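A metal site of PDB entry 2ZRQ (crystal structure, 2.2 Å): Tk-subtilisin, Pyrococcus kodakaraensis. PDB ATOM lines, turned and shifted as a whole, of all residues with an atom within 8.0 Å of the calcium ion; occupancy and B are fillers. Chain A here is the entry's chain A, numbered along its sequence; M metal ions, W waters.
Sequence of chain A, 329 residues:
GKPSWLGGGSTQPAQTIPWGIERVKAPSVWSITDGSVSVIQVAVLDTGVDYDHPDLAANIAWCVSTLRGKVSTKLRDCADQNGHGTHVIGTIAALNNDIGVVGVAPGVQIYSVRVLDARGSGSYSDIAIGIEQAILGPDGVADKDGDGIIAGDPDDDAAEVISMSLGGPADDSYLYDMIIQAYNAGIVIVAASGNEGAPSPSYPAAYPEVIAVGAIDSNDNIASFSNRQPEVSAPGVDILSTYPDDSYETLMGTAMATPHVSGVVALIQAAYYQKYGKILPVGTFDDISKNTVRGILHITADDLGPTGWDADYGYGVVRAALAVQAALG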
ATOM      1  N   TRP A  62      23.859 -31.568  -6.565  1.00  0.00           N
ATOM      2  CA  TRP A  62      22.636 -31.900  -5.822  1.00  0.00           C
ATOM      3  C   TRP A  62      22.640 -33.362  -5.479  1.00  0.00           C
ATOM      4  O   TRP A  62      23.063 -34.218  -6.275  1.00  0.00           O
ATOM      5  CB  TRP A  62      21.420 -31.576  -6.691  1.00  0.00           C
ATOM      6  CG  TRP A  62      20.035 -31.577  -6.073  1.00  0.00           C
ATOM      7  CD1 TRP A  62      19.635 -31.100  -4.810  1.00  0.00           C
ATOM      8  CD2 TRP A  62      18.830 -31.975  -6.745  1.00  0.00           C
ATOM      9  NE1 TRP A  62      18.266 -31.232  -4.684  1.00  0.00           N
ATOM     10  CE2 TRP A  62      17.748 -31.741  -5.847  1.00  0.00           C
ATOM     11  CE3 TRP A  62      18.567 -32.513  -8.022  1.00  0.00           C
ATOM     12  CZ2 TRP A  62      16.408 -32.048  -6.194  1.00  0.00           C
ATOM     13  CZ3 TRP A  62      17.217 -32.786  -8.366  1.00  0.00           C
ATOM     14  CH2 TRP A  62      16.175 -32.578  -7.451  1.00  0.00           C
ATOM     15  N   TYR A 111      23.850 -34.323 -10.626  1.00  0.00           N
ATOM     16  CA  TYR A 111      22.765 -34.554  -9.639  1.00  0.00           C
ATOM     17  C   TYR A 111      22.751 -36.045  -9.254  1.00  0.00           C
ATOM     18  O   TYR A 111      22.565 -36.921 -10.105  1.00  0.00           O
ATOM     19  CB  TYR A 111      21.373 -34.166 -10.167  1.00  0.00           C
ATOM     20  CG  TYR A 111      21.171 -32.714 -10.587  1.00  0.00           C
ATOM     21  CD1 TYR A 111      21.995 -31.692 -10.093  1.00  0.00           C
ATOM     22  CD2 TYR A 111      20.127 -32.373 -11.447  1.00  0.00           C
ATOM     23  CE1 TYR A 111      21.738 -30.337 -10.429  1.00  0.00           C
ATOM     24  CE2 TYR A 111      19.873 -31.079 -11.803  1.00  0.00           C
ATOM     25  CZ  TYR A 111      20.679 -30.045 -11.301  1.00  0.00           C
ATOM     26  OH  TYR A 111      20.415 -28.735 -11.678  1.00  0.00           O
ATOM     27  N   GLU A 132      11.232 -37.506 -12.449  1.00  0.00           N
ATOM     28  CA  GLU A 132      10.590 -36.220 -12.219  1.00  0.00           C
ATOM     29  C   GLU A 132      11.513 -35.183 -11.559  1.00  0.00           C
ATOM     30  O   GLU A 132      11.527 -34.032 -11.970  1.00  0.00           O
ATOM     31  CB  GLU A 132       9.357 -36.433 -11.313  1.00  0.00           C
ATOM     32  CG  GLU A 132       8.525 -35.156 -11.010  1.00  0.00           C
ATOM     33  CD  GLU A 132       7.165 -35.476 -10.356  1.00  0.00           C
ATOM     34  OE1 GLU A 132       6.129 -35.082 -10.921  1.00  0.00           O
ATOM     35  OE2 GLU A 132       7.133 -36.171  -9.316  1.00  0.00           O
ATOM     36  N   GLN A 133      12.253 -35.602 -10.523  1.00  0.00           N
ATOM     37  CA  GLN A 133      13.233 -34.756  -9.837  1.00  0.00           C
ATOM     38  C   GLN A 133      14.330 -34.211 -10.756  1.00  0.00           C
ATOM     39  O   GLN A 133      14.719 -33.084 -10.617  1.00  0.00           O
ATOM     40  CB  GLN A 133      13.882 -35.502  -8.639  1.00  0.00           C
ATOM     41  CG  GLN A 133      12.897 -35.730  -7.488  1.00  0.00           C
ATOM     42  CD  GLN A 133      12.182 -34.421  -7.064  1.00  0.00           C
ATOM     43  OE1 GLN A 133      12.825 -33.440  -6.774  1.00  0.00           O
ATOM     44  NE2 GLN A 133      10.864 -34.438  -7.062  1.00  0.00           N
ATOM     45  N   ALA A 134      14.806 -35.042 -11.691  1.00  0.00           N
ATOM     46  CA  ALA A 134      15.807 -34.663 -12.675  1.00  0.00           C
ATOM     47  C   ALA A 134      15.300 -33.527 -13.579  1.00  0.00           C
ATOM     48  O   ALA A 134      16.086 -32.664 -13.974  1.00  0.00           O
ATOM     49  CB  ALA A 134      16.244 -35.911 -13.533  1.00  0.00           C
ATOM     50  N   ILE A 135      13.987 -33.532 -13.857  1.00  0.00           N
ATOM     51  CA  ILE A 135      13.320 -32.523 -14.690  1.00  0.00           C
ATOM     52  C   ILE A 135      13.101 -31.231 -13.881  1.00  0.00           C
ATOM     53  O   ILE A 135      13.415 -30.157 -14.348  1.00  0.00           O
ATOM     54  CB  ILE A 135      11.930 -33.046 -15.276  1.00  0.00           C
ATOM     55  CG1 ILE A 135      12.138 -34.297 -16.134  1.00  0.00           C
ATOM     56  CG2 ILE A 135      11.196 -31.941 -16.080  1.00  0.00           C
ATOM     57  CD1 ILE A 135      10.860 -35.099 -16.485  1.00  0.00           C
ATOM     58  N   LEU A 136      12.569 -31.375 -12.685  1.00  0.00           N
ATOM     59  CA  LEU A 136      12.277 -30.265 -11.811  1.00  0.00           C
ATOM     60  C   LEU A 136      13.542 -29.648 -11.274  1.00  0.00           C
ATOM     61  O   LEU A 136      13.624 -28.430 -11.141  1.00  0.00           O
ATOM     62  CB  LEU A 136      11.402 -30.715 -10.635  1.00  0.00           C
ATOM     63  CG  LEU A 136       9.976 -31.205 -10.921  1.00  0.00           C
ATOM     64  CD1 LEU A 136       9.341 -31.760  -9.634  1.00  0.00           C
ATOM     65  CD2 LEU A 136       9.127 -30.092 -11.503  1.00  0.00           C
ATOM     66  N   GLY A 137      14.528 -30.484 -10.924  1.00  0.00           N
ATOM     67  CA  GLY A 137      15.824 -29.955 -10.499  1.00  0.00           C
ATOM     68  C   GLY A 137      15.730 -29.454  -9.074  1.00  0.00           C
ATOM     69  O   GLY A 137      14.658 -29.528  -8.478  1.00  0.00           O
ATOM     70  N   PRO A 138      16.856 -28.978  -8.506  1.00  0.00           N
ATOM     71  CA  PRO A 138      16.914 -28.551  -7.104  1.00  0.00           C
ATOM     72  C   PRO A 138      15.877 -27.524  -6.701  1.00  0.00           C
ATOM     73  O   PRO A 138      15.460 -27.543  -5.547  1.00  0.00           O
ATOM     74  CB  PRO A 138      18.315 -27.977  -6.979  1.00  0.00           C
ATOM     75  CG  PRO A 138      19.100 -28.667  -8.025  1.00  0.00           C
ATOM     76  CD  PRO A 138      18.176 -28.842  -9.160  1.00  0.00           C
ATOM     77  N   ASP A 139      15.436 -26.652  -7.621  1.00  0.00           N
ATOM     78  CA  ASP A 139      14.455 -25.625  -7.234  1.00  0.00           C
ATOM     79  C   ASP A 139      13.011 -26.129  -7.170  1.00  0.00           C
ATOM     80  O   ASP A 139      12.172 -25.386  -6.697  1.00  0.00           O
ATOM     81  CB  ASP A 139      14.589 -24.319  -8.048  1.00  0.00           C
ATOM     82  CG  ASP A 139      14.200 -24.481  -9.538  1.00  0.00           C
ATOM     83  OD1 ASP A 139      13.589 -25.489  -9.929  1.00  0.00           O
ATOM     84  OD2 ASP A 139      14.504 -23.610 -10.358  1.00  0.00           O
ATOM     85  N   GLY A 140      12.748 -27.372  -7.620  1.00  0.00           N
ATOM     86  CA  GLY A 140      11.412 -27.995  -7.651  1.00  0.00           C
ATOM     87  C   GLY A 140      10.401 -27.474  -8.693  1.00  0.00           C
ATOM     88  O   GLY A 140       9.226 -27.840  -8.647  1.00  0.00           O
ATOM     89  N   VAL A 141      10.861 -26.603  -9.596  1.00  0.00           N
ATOM     90  CA  VAL A 141      10.010 -26.007 -10.644  1.00  0.00           C
ATOM     91  C   VAL A 141      10.581 -26.383 -12.042  1.00  0.00           C
ATOM     92  O   VAL A 141      11.799 -26.269 -12.255  1.00  0.00           O
ATOM     93  CB  VAL A 141       9.976 -24.449 -10.516  1.00  0.00           C
ATOM     94  CG1 VAL A 141       9.084 -23.852 -11.554  1.00  0.00           C
ATOM     95  CG2 VAL A 141       9.501 -23.977  -9.117  1.00  0.00           C
ATOM     96  N   ALA A 142       9.734 -26.837 -12.972  1.00  0.00           N
ATOM     97  CA  ALA A 142      10.237 -27.222 -14.307  1.00  0.00           C
ATOM     98  C   ALA A 142      10.733 -26.040 -15.147  1.00  0.00           C
ATOM     99  O   ALA A 142      11.898 -25.987 -15.575  1.00  0.00           O
ATOM    100  CB  ALA A 142       9.192 -28.052 -15.102  1.00  0.00           C
ATOM    101  N   ASP A 143       9.864 -25.062 -15.347  1.00  0.00           N
ATOM    102  CA  ASP A 143      10.162 -23.983 -16.271  1.00  0.00           C
ATOM    103  C   ASP A 143       9.936 -22.691 -15.516  1.00  0.00           C
ATOM    104  O   ASP A 143       8.907 -22.034 -15.698  1.00  0.00           O
ATOM    105  CB  ASP A 143       9.261 -24.084 -17.502  1.00  0.00           C
ATOM    106  CG  ASP A 143       9.498 -22.963 -18.509  1.00  0.00           C
ATOM    107  OD1 ASP A 143      10.554 -22.315 -18.508  1.00  0.00           O
ATOM    108  OD2 ASP A 143       8.617 -22.738 -19.343  1.00  0.00           O
ATOM    109  N   LYS A 144      10.900 -22.329 -14.664  1.00  0.00           N
ATOM    110  CA  LYS A 144      10.710 -21.230 -13.732  1.00  0.00           C
ATOM    111  C   LYS A 144      10.449 -19.866 -14.393  1.00  0.00           C
ATOM    112  O   LYS A 144       9.656 -19.094 -13.882  1.00  0.00           O
ATOM    113  CB  LYS A 144      11.780 -21.196 -12.612  1.00  0.00           C
ATOM    114  CG  LYS A 144      13.168 -20.648 -12.978  1.00  0.00           C
ATOM    115  CD  LYS A 144      13.826 -19.935 -11.731  1.00  0.00           C
ATOM    116  CE  LYS A 144      15.282 -19.434 -12.013  1.00  0.00           C
ATOM    117  NZ  LYS A 144      15.463 -18.415 -13.158  1.00  0.00           N
ATOM    118  N   ILE A 150      13.351 -26.025 -21.034  1.00  0.00           N
ATOM    119  CA  ILE A 150      13.741 -26.644 -19.760  1.00  0.00           C
ATOM    120  C   ILE A 150      15.209 -27.125 -19.837  1.00  0.00           C
ATOM    121  O   ILE A 150      16.084 -26.517 -19.220  1.00  0.00           O
ATOM    122  CB  ILE A 150      12.744 -27.798 -19.388  1.00  0.00           C
ATOM    123  CG1 ILE A 150      11.373 -27.224 -19.028  1.00  0.00           C
ATOM    124  CG2 ILE A 150      13.233 -28.616 -18.257  1.00  0.00           C
ATOM    125  CD1 ILE A 150      10.193 -28.175 -19.271  1.00  0.00           C
ATOM    126  N   ASP A 155      18.380 -20.391 -17.218  1.00  0.00           N
ATOM    127  CA  ASP A 155      17.408 -19.893 -16.224  1.00  0.00           C
ATOM    128  C   ASP A 155      16.669 -21.034 -15.496  1.00  0.00           C
ATOM    129  O   ASP A 155      15.959 -20.790 -14.536  1.00  0.00           O
ATOM    130  CB  ASP A 155      16.404 -18.908 -16.880  1.00  0.00           C
ATOM    131  CG  ASP A 155      17.119 -17.767 -17.626  1.00  0.00           C
ATOM    132  OD1 ASP A 155      17.923 -17.020 -16.974  1.00  0.00           O
ATOM    133  OD2 ASP A 155      16.931 -17.643 -18.854  1.00  0.00           O
ATOM    134  N   ASP A 156      16.817 -22.266 -15.968  1.00  0.00           N
ATOM    135  CA  ASP A 156      16.310 -23.429 -15.221  1.00  0.00           C
ATOM    136  C   ASP A 156      17.434 -24.314 -14.725  1.00  0.00           C
ATOM    137  O   ASP A 156      18.590 -24.107 -15.077  1.00  0.00           O
ATOM    138  CB  ASP A 156      15.289 -24.189 -16.040  1.00  0.00           C
ATOM    139  CG  ASP A 156      13.973 -23.485 -16.052  1.00  0.00           C
ATOM    140  OD1 ASP A 156      13.348 -23.371 -14.976  1.00  0.00           O
ATOM    141  OD2 ASP A 156      13.574 -23.016 -17.134  1.00  0.00           O
ATOM    142  N   ASP A 157      17.091 -25.306 -13.894  1.00  0.00           N
ATOM    143  CA  ASP A 157      18.112 -26.213 -13.367  1.00  0.00           C
ATOM    144  C   ASP A 157      17.793 -27.712 -13.666  1.00  0.00           C
ATOM    145  O   ASP A 157      18.277 -28.599 -12.968  1.00  0.00           O
ATOM    146  CB  ASP A 157      18.316 -25.956 -11.870  1.00  0.00           C
ATOM    147  CG  ASP A 157      17.049 -26.190 -11.050  1.00  0.00           C
ATOM    148  OD1 ASP A 157      17.029 -25.840  -9.872  1.00  0.00           O
ATOM    149  OD2 ASP A 157      16.063 -26.732 -11.602  1.00  0.00           O
ATOM    150  N   ALA A 158      16.972 -27.965 -14.681  1.00  0.00           N
ATOM    151  CA  ALA A 158      16.755 -29.316 -15.189  1.00  0.00           C
ATOM    152  C   ALA A 158      18.061 -29.937 -15.671  1.00  0.00           C
ATOM    153  O   ALA A 158      18.927 -29.237 -16.228  1.00  0.00           O
ATOM    154  CB  ALA A 158      15.744 -29.277 -16.375  1.00  0.00           C
ATOM    155  N   ALA A 159      18.207 -31.238 -15.451  1.00  0.00           N
ATOM    156  CA  ALA A 159      19.314 -31.984 -16.060  1.00  0.00           C
ATOM    157  C   ALA A 159      19.110 -32.044 -17.577  1.00  0.00           C
ATOM    158  O   ALA A 159      17.971 -31.909 -18.056  1.00  0.00           O
ATOM    159  CB  ALA A 159      19.404 -33.416 -15.458  1.00  0.00           C
HETATM  160 CA    CA M   1      13.864 -26.449 -11.938  1.00  0.00          CA
HETATM  161  O   HOH W   1      13.785 -27.411 -14.098  1.00  0.00           O
HETATM  162  O   HOH W   2      14.335 -24.300 -12.780  1.00  0.00           O
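Water W1 lies within hydrogen-bond range of O of Ile 135 (2.8 Å), O of Ala 142 (2.8 Å) and N of Ala 158 (3.3 Å).
Water W2 lies within hydrogen-bond range of the side-chain carboxylate (OD2) of Asp 139 (2.5 Å), the side-chain carboxylate (OD1) of Asp 156 (2.6 Å) and the backbone NH (N) of Asp 157 (3.1 Å).
The side-chain hydroxyl (OH) of Tyr 111 is in hydrogen-bond range of the backbone carbonyl oxygen (O) of Asp 157 (2.5 Å).
Within 4 Å of the calcium ion: Leu 136, Asp 139, Val 141 and Asp 157.
The calcium ion is bound by O of Val 141, O of Leu 136, OD2 of Asp 157, OD1 of Asp 139, water W2 and water W1.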
